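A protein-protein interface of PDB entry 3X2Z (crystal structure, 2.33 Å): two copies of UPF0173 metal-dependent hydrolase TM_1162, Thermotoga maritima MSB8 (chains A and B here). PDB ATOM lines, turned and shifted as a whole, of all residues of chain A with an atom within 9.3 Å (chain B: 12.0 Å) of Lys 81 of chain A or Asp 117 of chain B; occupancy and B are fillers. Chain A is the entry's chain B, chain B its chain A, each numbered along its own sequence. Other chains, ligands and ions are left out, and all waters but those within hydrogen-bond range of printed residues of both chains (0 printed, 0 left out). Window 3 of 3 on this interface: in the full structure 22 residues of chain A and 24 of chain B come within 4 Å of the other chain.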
ATOM      1  N   VAL A  59      29.231 -27.301  -1.646  1.00  0.00           N
ATOM      2  CA  VAL A  59      30.246 -27.054  -0.619  1.00  0.00           C
ATOM      3  C   VAL A  59      31.606 -26.741  -1.249  1.00  0.00           C
ATOM      4  O   VAL A  59      32.204 -25.705  -0.961  1.00  0.00           O
ATOM      5  CB  VAL A  59      30.376 -28.251   0.351  1.00  0.00           C
ATOM      6  CG1 VAL A  59      31.511 -28.034   1.346  1.00  0.00           C
ATOM      7  CG2 VAL A  59      29.068 -28.474   1.099  1.00  0.00           C
ATOM      8  N   LYS A  63      33.376 -22.922  -1.124  1.00  0.00           N
ATOM      9  CA  LYS A  63      34.669 -22.736  -0.454  1.00  0.00           C
ATOM     10  C   LYS A  63      35.776 -22.235  -1.380  1.00  0.00           C
ATOM     11  O   LYS A  63      36.510 -21.312  -1.028  1.00  0.00           O
ATOM     12  CB  LYS A  63      35.115 -24.043   0.201  1.00  0.00           C
ATOM     13  CG  LYS A  63      34.437 -24.319   1.528  1.00  0.00           C
ATOM     14  CD  LYS A  63      34.784 -25.705   2.040  1.00  0.00           C
ATOM     15  CE  LYS A  63      34.591 -25.793   3.540  1.00  0.00           C
ATOM     16  NZ  LYS A  63      34.708 -27.191   4.036  1.00  0.00           N
ATOM     17  N   TYR A  73      16.351 -22.179   5.132  1.00  0.00           N
ATOM     18  CA  TYR A  73      16.978 -22.138   6.453  1.00  0.00           C
ATOM     19  C   TYR A  73      17.638 -23.462   6.854  1.00  0.00           C
ATOM     20  O   TYR A  73      18.767 -23.474   7.346  1.00  0.00           O
ATOM     21  CB  TYR A  73      15.940 -21.717   7.497  1.00  0.00           C
ATOM     22  CG  TYR A  73      16.360 -21.938   8.934  1.00  0.00           C
ATOM     23  CD1 TYR A  73      17.318 -21.127   9.538  1.00  0.00           C
ATOM     24  CD2 TYR A  73      15.788 -22.954   9.695  1.00  0.00           C
ATOM     25  CE1 TYR A  73      17.700 -21.327  10.856  1.00  0.00           C
ATOM     26  CE2 TYR A  73      16.161 -23.163  11.013  1.00  0.00           C
ATOM     27  CZ  TYR A  73      17.116 -22.348  11.589  1.00  0.00           C
ATOM     28  OH  TYR A  73      17.484 -22.559  12.899  1.00  0.00           O
ATOM     29  N   GLU A  74      16.941 -24.569   6.626  1.00  0.00           N
ATOM     30  CA  GLU A  74      17.427 -25.889   7.039  1.00  0.00           C
ATOM     31  C   GLU A  74      18.649 -26.338   6.228  1.00  0.00           C
ATOM     32  O   GLU A  74      19.582 -26.923   6.776  1.00  0.00           O
ATOM     33  CB  GLU A  74      16.316 -26.939   6.940  1.00  0.00           C
ATOM     34  CG  GLU A  74      15.225 -26.805   8.000  1.00  0.00           C
ATOM     35  CD  GLU A  74      14.140 -25.802   7.642  1.00  0.00           C
ATOM     36  OE1 GLU A  74      14.201 -25.199   6.546  1.00  0.00           O
ATOM     37  OE2 GLU A  74      13.215 -25.613   8.460  1.00  0.00           O
ATOM     38  N   ILE A  75      18.635 -26.065   4.926  1.00  0.00           N
ATOM     39  CA  ILE A  75      19.773 -26.380   4.060  1.00  0.00           C
ATOM     40  C   ILE A  75      20.975 -25.498   4.413  1.00  0.00           C
ATOM     41  O   ILE A  75      22.107 -25.975   4.455  1.00  0.00           O
ATOM     42  CB  ILE A  75      19.412 -26.233   2.563  1.00  0.00           C
ATOM     43  CG1 ILE A  75      18.404 -27.314   2.164  1.00  0.00           C
ATOM     44  CG2 ILE A  75      20.662 -26.329   1.686  1.00  0.00           C
ATOM     45  CD1 ILE A  75      17.835 -27.169   0.767  1.00  0.00           C
ATOM     46  N   CYS A  76      20.720 -24.219   4.669  1.00  0.00           N
ATOM     47  CA  CYS A  76      21.780 -23.272   5.034  1.00  0.00           C
ATOM     48  C   CYS A  76      22.424 -23.597   6.385  1.00  0.00           C
ATOM     49  O   CYS A  76      23.601 -23.307   6.600  1.00  0.00           O
ATOM     50  CB  CYS A  76      21.243 -21.841   5.039  1.00  0.00           C
ATOM     51  SG  CYS A  76      20.974 -21.174   3.380  1.00  0.00           S
ATOM     52  N   HIS A  77      21.651 -24.192   7.286  1.00  0.00           N
ATOM     53  CA  HIS A  77      22.174 -24.666   8.566  1.00  0.00           C
ATOM     54  C   HIS A  77      23.163 -25.809   8.343  1.00  0.00           C
ATOM     55  O   HIS A  77      24.269 -25.802   8.881  1.00  0.00           O
ATOM     56  CB  HIS A  77      21.030 -25.132   9.467  1.00  0.00           C
ATOM     57  CG  HIS A  77      21.485 -25.758  10.748  1.00  0.00           C
ATOM     58  ND1 HIS A  77      21.607 -27.122  10.905  1.00  0.00           N
ATOM     59  CD2 HIS A  77      21.852 -25.211  11.932  1.00  0.00           C
ATOM     60  CE1 HIS A  77      22.025 -27.389  12.129  1.00  0.00           C
ATOM     61  NE2 HIS A  77      22.181 -26.246  12.773  1.00  0.00           N
ATOM     62  N   TYR A  78      22.745 -26.787   7.546  1.00  0.00           N
ATOM     63  CA  TYR A  78      23.586 -27.931   7.191  1.00  0.00           C
ATOM     64  C   TYR A  78      24.888 -27.483   6.529  1.00  0.00           C
ATOM     65  O   TYR A  78      25.966 -27.968   6.873  1.00  0.00           O
ATOM     66  CB  TYR A  78      22.817 -28.873   6.260  1.00  0.00           C
ATOM     67  CG  TYR A  78      23.646 -29.973   5.628  1.00  0.00           C
ATOM     68  CD1 TYR A  78      23.852 -31.182   6.284  1.00  0.00           C
ATOM     69  CD2 TYR A  78      24.207 -29.809   4.362  1.00  0.00           C
ATOM     70  CE1 TYR A  78      24.600 -32.193   5.703  1.00  0.00           C
ATOM     71  CE2 TYR A  78      24.957 -30.813   3.774  1.00  0.00           C
ATOM     72  CZ  TYR A  78      25.149 -32.004   4.447  1.00  0.00           C
ATOM     73  OH  TYR A  78      25.895 -33.006   3.867  1.00  0.00           O
ATOM     74  N   LEU A  79      24.775 -26.559   5.579  1.00  0.00           N
ATOM     75  CA  LEU A  79      25.940 -26.018   4.879  1.00  0.00           C
ATOM     76  C   LEU A  79      26.828 -25.166   5.784  1.00  0.00           C
ATOM     77  O   LEU A  79      28.055 -25.201   5.666  1.00  0.00           O
ATOM     78  CB  LEU A  79      25.499 -25.198   3.664  1.00  0.00           C
ATOM     79  CG  LEU A  79      24.842 -25.981   2.526  1.00  0.00           C
ATOM     80  CD1 LEU A  79      24.330 -25.014   1.474  1.00  0.00           C
ATOM     81  CD2 LEU A  79      25.799 -26.984   1.902  1.00  0.00           C
ATOM     82  N   GLY A  80      26.208 -24.411   6.687  1.00  0.00           N
ATOM     83  CA  GLY A  80      26.940 -23.566   7.631  1.00  0.00           C
ATOM     84  C   GLY A  80      27.897 -24.351   8.515  1.00  0.00           C
ATOM     85  O   GLY A  80      29.002 -23.892   8.807  1.00  0.00           O
ATOM     86  N   LYS A  81      27.476 -25.545   8.927  1.00  0.00           N
ATOM     87  CA  LYS A  81      28.296 -26.413   9.772  1.00  0.00           C
ATOM     88  C   LYS A  81      29.503 -26.990   9.024  1.00  0.00           C
ATOM     89  O   LYS A  81      30.473 -27.419   9.649  1.00  0.00           O
ATOM     90  CB  LYS A  81      27.449 -27.546  10.356  1.00  0.00           C
ATOM     91  CG  LYS A  81      26.345 -27.073  11.290  1.00  0.00           C
ATOM     92  CD  LYS A  81      25.875 -28.166  12.239  1.00  0.00           C
ATOM     93  CE  LYS A  81      25.382 -29.402  11.505  1.00  0.00           C
ATOM     94  NZ  LYS A  81      24.883 -30.439  12.449  1.00  0.00           N
ATOM     95  N   LYS A  82      29.431 -27.002   7.694  1.00  0.00           N
ATOM     96  CA  LYS A  82      30.556 -27.398   6.842  1.00  0.00           C
ATOM     97  C   LYS A  82      31.445 -26.221   6.417  1.00  0.00           C
ATOM     98  O   LYS A  82      32.305 -26.377   5.552  1.00  0.00           O
ATOM     99  CB  LYS A  82      30.037 -28.128   5.604  1.00  0.00           C
ATOM    100  CG  LYS A  82      29.306 -29.413   5.936  1.00  0.00           C
ATOM    101  CD  LYS A  82      29.193 -30.328   4.731  1.00  0.00           C
ATOM    102  CE  LYS A  82      28.431 -31.599   5.072  1.00  0.00           C
ATOM    103  NZ  LYS A  82      29.047 -32.405   6.164  1.00  0.00           N
ATOM    104  N   GLY A  83      31.235 -25.054   7.022  1.00  0.00           N
ATOM    105  CA  GLY A  83      32.078 -23.878   6.779  1.00  0.00           C
ATOM    106  C   GLY A  83      31.706 -23.048   5.560  1.00  0.00           C
ATOM    107  O   GLY A  83      32.497 -22.219   5.106  1.00  0.00           O
ATOM    108  N   VAL A  84      30.500 -23.259   5.040  1.00  0.00           N
ATOM    109  CA  VAL A  84      30.024 -22.555   3.845  1.00  0.00           C
ATOM    110  C   VAL A  84      29.288 -21.272   4.234  1.00  0.00           C
ATOM    111  O   VAL A  84      28.500 -21.265   5.178  1.00  0.00           O
ATOM    112  CB  VAL A  84      29.082 -23.453   3.010  1.00  0.00           C
ATOM    113  CG1 VAL A  84      28.476 -22.690   1.838  1.00  0.00           C
ATOM    114  CG2 VAL A  84      29.826 -24.681   2.508  1.00  0.00           C
ATOM    115  N   LYS A  85      29.557 -20.194   3.500  1.00  0.00           N
ATOM    116  CA  LYS A  85      28.824 -18.935   3.659  1.00  0.00           C
ATOM    117  C   LYS A  85      27.419 -19.072   3.081  1.00  0.00           C
ATOM    118  O   LYS A  85      27.242 -19.609   1.986  1.00  0.00           O
ATOM    119  CB  LYS A  85      29.546 -17.789   2.951  1.00  0.00           C
ATOM    120  CG  LYS A  85      30.836 -17.346   3.617  1.00  0.00           C
ATOM    121  CD  LYS A  85      31.397 -16.104   2.943  1.00  0.00           C
ATOM    122  CE  LYS A  85      32.688 -15.646   3.603  1.00  0.00           C
ATOM    123  NZ  LYS A  85      33.230 -14.414   2.965  1.00  0.00           N
ATOM    124  N   THR A  86      26.425 -18.569   3.809  1.00  0.00           N
ATOM    125  CA  THR A  86      25.026 -18.722   3.409  1.00  0.00           C
ATOM    126  C   THR A  86      24.206 -17.446   3.563  1.00  0.00           C
ATOM    127  O   THR A  86      24.498 -16.602   4.409  1.00  0.00           O
ATOM    128  CB  THR A  86      24.316 -19.812   4.237  1.00  0.00           C
ATOM    129  OG1 THR A  86      24.286 -19.430   5.618  1.00  0.00           O
ATOM    130  CG2 THR A  86      25.016 -21.157   4.096  1.00  0.00           C
ATOM    131  N   ASP A 115      23.482 -37.638   4.192  1.00  0.00           N
ATOM    132  CA  ASP A 115      24.803 -37.488   4.807  1.00  0.00           C
ATOM    133  C   ASP A 115      25.229 -38.827   5.406  1.00  0.00           C
ATOM    134  O   ASP A 115      24.708 -39.253   6.440  1.00  0.00           O
ATOM    135  CB  ASP A 115      24.785 -36.394   5.881  1.00  0.00           C
ATOM    136  CG  ASP A 115      26.184 -35.950   6.301  1.00  0.00           C
ATOM    137  OD1 ASP A 115      27.177 -36.608   5.920  1.00  0.00           O
ATOM    138  OD2 ASP A 115      26.293 -34.936   7.019  1.00  0.00           O
ATOM    139  N   ILE A 120      19.096 -36.373   6.514  1.00  0.00           N
ATOM    140  CA  ILE A 120      18.931 -35.140   7.276  1.00  0.00           C
ATOM    141  C   ILE A 120      17.801 -34.290   6.686  1.00  0.00           C
ATOM    142  O   ILE A 120      17.626 -34.228   5.467  1.00  0.00           O
ATOM    143  CB  ILE A 120      20.253 -34.340   7.329  1.00  0.00           C
ATOM    144  CG1 ILE A 120      21.290 -35.117   8.151  1.00  0.00           C
ATOM    145  CG2 ILE A 120      20.034 -32.953   7.928  1.00  0.00           C
ATOM    146  CD1 ILE A 120      22.684 -34.520   8.139  1.00  0.00           C
ATOM    147  N   TYR B  78       8.244 -34.255  19.698  1.00  0.00           N
ATOM    148  CA  TYR B  78       9.422 -33.586  20.245  1.00  0.00           C
ATOM    149  C   TYR B  78       9.132 -33.020  21.636  1.00  0.00           C
ATOM    150  O   TYR B  78       9.895 -33.240  22.576  1.00  0.00           O
ATOM    151  CB  TYR B  78       9.878 -32.469  19.303  1.00  0.00           C
ATOM    152  CG  TYR B  78      10.986 -31.593  19.850  1.00  0.00           C
ATOM    153  CD1 TYR B  78      12.323 -31.972  19.738  1.00  0.00           C
ATOM    154  CD2 TYR B  78      10.699 -30.377  20.468  1.00  0.00           C
ATOM    155  CE1 TYR B  78      13.338 -31.168  20.230  1.00  0.00           C
ATOM    156  CE2 TYR B  78      11.708 -29.569  20.965  1.00  0.00           C
ATOM    157  CZ  TYR B  78      13.025 -29.967  20.841  1.00  0.00           C
ATOM    158  OH  TYR B  78      14.029 -29.166  21.335  1.00  0.00           O
ATOM    159  N   LYS B  82      10.083 -33.911  26.081  1.00  0.00           N
ATOM    160  CA  LYS B  82      10.492 -32.912  27.078  1.00  0.00           C
ATOM    161  C   LYS B  82       9.579 -32.898  28.309  1.00  0.00           C
ATOM    162  O   LYS B  82       9.831 -32.155  29.252  1.00  0.00           O
ATOM    163  CB  LYS B  82      10.496 -31.502  26.473  1.00  0.00           C
ATOM    164  CG  LYS B  82      11.296 -31.333  25.193  1.00  0.00           C
ATOM    165  CD  LYS B  82      12.797 -31.315  25.427  1.00  0.00           C
ATOM    166  CE  LYS B  82      13.501 -30.617  24.273  1.00  0.00           C
ATOM    167  NZ  LYS B  82      14.923 -31.026  24.117  1.00  0.00           N
ATOM    168  N   GLY B 112      11.881 -26.950  10.677  1.00  0.00           N
ATOM    169  CA  GLY B 112      13.042 -27.543  11.335  1.00  0.00           C
ATOM    170  C   GLY B 112      13.164 -27.124  12.791  1.00  0.00           C
ATOM    171  O   GLY B 112      13.084 -25.941  13.112  1.00  0.00           O
ATOM    172  N   ILE B 113      13.356 -28.101  13.673  1.00  0.00           N
ATOM    173  CA  ILE B 113      13.566 -27.837  15.095  1.00  0.00           C
ATOM    174  C   ILE B 113      15.057 -27.933  15.413  1.00  0.00           C
ATOM    175  O   ILE B 113      15.637 -29.021  15.380  1.00  0.00           O
ATOM    176  CB  ILE B 113      12.789 -28.830  15.984  1.00  0.00           C
ATOM    177  CG1 ILE B 113      11.288 -28.758  15.681  1.00  0.00           C
ATOM    178  CG2 ILE B 113      13.044 -28.538  17.459  1.00  0.00           C
ATOM    179  CD1 ILE B 113      10.486 -29.898  16.270  1.00  0.00           C
ATOM    180  N   LEU B 114      15.672 -26.794  15.718  1.00  0.00           N
ATOM    181  CA  LEU B 114      17.084 -26.759  16.082  1.00  0.00           C
ATOM    182  C   LEU B 114      17.266 -27.204  17.532  1.00  0.00           C
ATOM    183  O   LEU B 114      16.917 -26.475  18.461  1.00  0.00           O
ATOM    184  CB  LEU B 114      17.671 -25.358  15.881  1.00  0.00           C
ATOM    185  CG  LEU B 114      19.170 -25.209  16.180  1.00  0.00           C
ATOM    186  CD1 LEU B 114      20.012 -26.097  15.270  1.00  0.00           C
ATOM    187  CD2 LEU B 114      19.602 -23.758  16.050  1.00  0.00           C
ATOM    188  N   ASP B 115      17.807 -28.407  17.707  1.00  0.00           N
ATOM    189  CA  ASP B 115      18.092 -28.958  19.033  1.00  0.00           C
ATOM    190  C   ASP B 115      19.604 -29.063  19.222  1.00  0.00           C
ATOM    191  O   ASP B 115      20.234 -30.040  18.811  1.00  0.00           O
ATOM    192  CB  ASP B 115      17.422 -30.324  19.212  1.00  0.00           C
ATOM    193  CG  ASP B 115      17.359 -30.760  20.670  1.00  0.00           C
ATOM    194  OD1 ASP B 115      17.007 -29.928  21.534  1.00  0.00           O
ATOM    195  OD2 ASP B 115      17.645 -31.943  20.951  1.00  0.00           O
ATOM    196  N   GLY B 116      20.174 -28.035  19.846  1.00  0.00           N
ATOM    197  CA  GLY B 116      21.618 -27.910  19.984  1.00  0.00           C
ATOM    198  C   GLY B 116      22.271 -27.718  18.628  1.00  0.00           C
ATOM    199  O   GLY B 116      22.191 -26.640  18.035  1.00  0.00           O
ATOM    200  N   ASP B 117      22.904 -28.779  18.140  1.00  0.00           N
ATOM    201  CA  ASP B 117      23.592 -28.769  16.849  1.00  0.00           C
ATOM    202  C   ASP B 117      22.782 -29.447  15.734  1.00  0.00           C
ATOM    203  O   ASP B 117      23.128 -29.332  14.556  1.00  0.00           O
ATOM    204  CB  ASP B 117      24.948 -29.469  16.997  1.00  0.00           C
ATOM    205  CG  ASP B 117      25.919 -29.121  15.883  1.00  0.00           C
ATOM    206  OD1 ASP B 117      26.125 -27.916  15.620  1.00  0.00           O
ATOM    207  OD2 ASP B 117      26.486 -30.056  15.277  1.00  0.00           O
ATOM    208  N   SER B 118      21.705 -30.139  16.106  1.00  0.00           N
ATOM    209  CA  SER B 118      20.955 -30.986  15.177  1.00  0.00           C
ATOM    210  C   SER B 118      19.635 -30.356  14.736  1.00  0.00           C
ATOM    211  O   SER B 118      18.917 -29.770  15.546  1.00  0.00           O
ATOM    212  CB  SER B 118      20.666 -32.340  15.830  1.00  0.00           C
ATOM    213  OG  SER B 118      21.866 -32.990  16.202  1.00  0.00           O
ATOM    214  N   MET B 119      19.326 -30.494  13.447  1.00  0.00           N
ATOM    215  CA  MET B 119      18.052 -30.037  12.891  1.00  0.00           C
ATOM    216  C   MET B 119      17.051 -31.188  12.887  1.00  0.00           C
ATOM    217  O   MET B 119      17.094 -32.059  12.019  1.00  0.00           O
ATOM    218  CB  MET B 119      18.239 -29.495  11.472  1.00  0.00           C
ATOM    219  CG  MET B 119      17.041 -28.719  10.937  1.00  0.00           C
ATOM    220  SD  MET B 119      16.696 -27.197  11.846  1.00  0.00           S
ATOM    221  CE  MET B 119      18.115 -26.196  11.410  1.00  0.00           C
ATOM    222  N   ILE B 120      16.155 -31.184  13.869  1.00  0.00           N
ATOM    223  CA  ILE B 120      15.130 -32.218  13.994  1.00  0.00           C
ATOM    224  C   ILE B 120      13.934 -31.902  13.090  1.00  0.00           C
ATOM    225  O   ILE B 120      13.546 -30.743  12.932  1.00  0.00           O
ATOM    226  CB  ILE B 120      14.688 -32.389  15.469  1.00  0.00           C
ATOM    227  CG1 ILE B 120      15.877 -32.898  16.300  1.00  0.00           C
ATOM    228  CG2 ILE B 120      13.493 -33.334  15.582  1.00  0.00           C
ATOM    229  CD1 ILE B 120      15.557 -33.262  17.737  1.00  0.00           C
ATOM    230  N   TYR B 121      13.364 -32.948  12.497  1.00  0.00           N
ATOM    231  CA  TYR B 121      12.200 -32.821  11.627  1.00  0.00           C
ATOM    232  C   TYR B 121      10.949 -32.492  12.437  1.00  0.00           C
ATOM    233  O   TYR B 121      10.524 -33.287  13.271  1.00  0.00           O
ATOM    234  CB  TYR B 121      11.976 -34.120  10.847  1.00  0.00           C
ATOM    235  CG  TYR B 121      10.720 -34.112  10.001  1.00  0.00           C
ATOM    236  CD1 TYR B 121      10.509 -33.119   9.050  1.00  0.00           C
ATOM    237  CD2 TYR B 121       9.746 -35.095  10.148  1.00  0.00           C
ATOM    238  CE1 TYR B 121       9.364 -33.101   8.272  1.00  0.00           C
ATOM    239  CE2 TYR B 121       8.600 -35.085   9.370  1.00  0.00           C
ATOM    240  CZ  TYR B 121       8.414 -34.089   8.433  1.00  0.00           C
ATOM    241  OH  TYR B 121       7.274 -34.075   7.663  1.00  0.00           O
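The backbone NH (N) of Gly 112 of chain B sits at hydrogen-bond distance from the side-chain carboxylate (OE2) of Glu 74 of chain A (2.9 Å). The side-chain carboxylate (OD2) of Asp 117 of chain B is in salt-bridge range of the side-chain amino group (NZ) of Lys 81 of chain A.
Among the printed residues, pairs that only touch across the chains: Tyr 73 of chain A with Leu 114 of chain B (3.98 Å), Tyr 73 of chain A with Met 119 of chain B (3.6 Å), Glu 74 of chain A with Met 119 of chain B (3.9 Å), His 77 of chain A with Leu 114 of chain B (3.3 Å), His 77 of chain A with Asp 117 of chain B (3.3 Å) and His 77 of chain A with Met 119 of chain B (3.5 Å).
Of chain B, only Asp 117 (3.0 Å) comes within 4 Å of Lys 81 of chain A. His 77 of chain A touches just these residues of chain B: Leu 114 (3.3 Å), Asp 117 (3.3 Å) and Met 119 (3.5 Å). No residue of chain B comes within 4 Å of Gly 80 of chain A. No residue of chain B comes within 4 Å of Lys 82 of chain A. Val 84 of chain A touches none of the printed residues of chain B. No residue of chain A comes within 4 Å of Gly 116 of chain B. Of the printed residues of chain A, Gly 112 of chain B touches Glu 74. Printed residues of chain B within 4 Å of Tyr 73 of chain A: Leu 114 (3.98 Å) and Met 119 (3.6 Å). The nearest residue of chain B that does not touch Lys 81 of chain A is Ser 118 of chain B (4.8 Å). The nearest residue of chain A that does not touch Asp 117 of chain B is Tyr 78 of chain A (7.5 Å). The nearest printed residue of chain B that does not touch Glu 74 of chain A is Ile 113 of chain B (5.8 Å).
Of the 12 printed residues of chain B, 4 touch a printed residue of chain A. Hydrophobic or aromatic side chains of chain B that line the printed part of chain A: Leu 114 and Met 119. Hydrophobic or aromatic side chains of chain A within 4 Å of the printed part of chain B: Tyr 73 and His 77. Among the printed residues, 8 pairs touch across the chains.
4 positions are printed for both chains.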
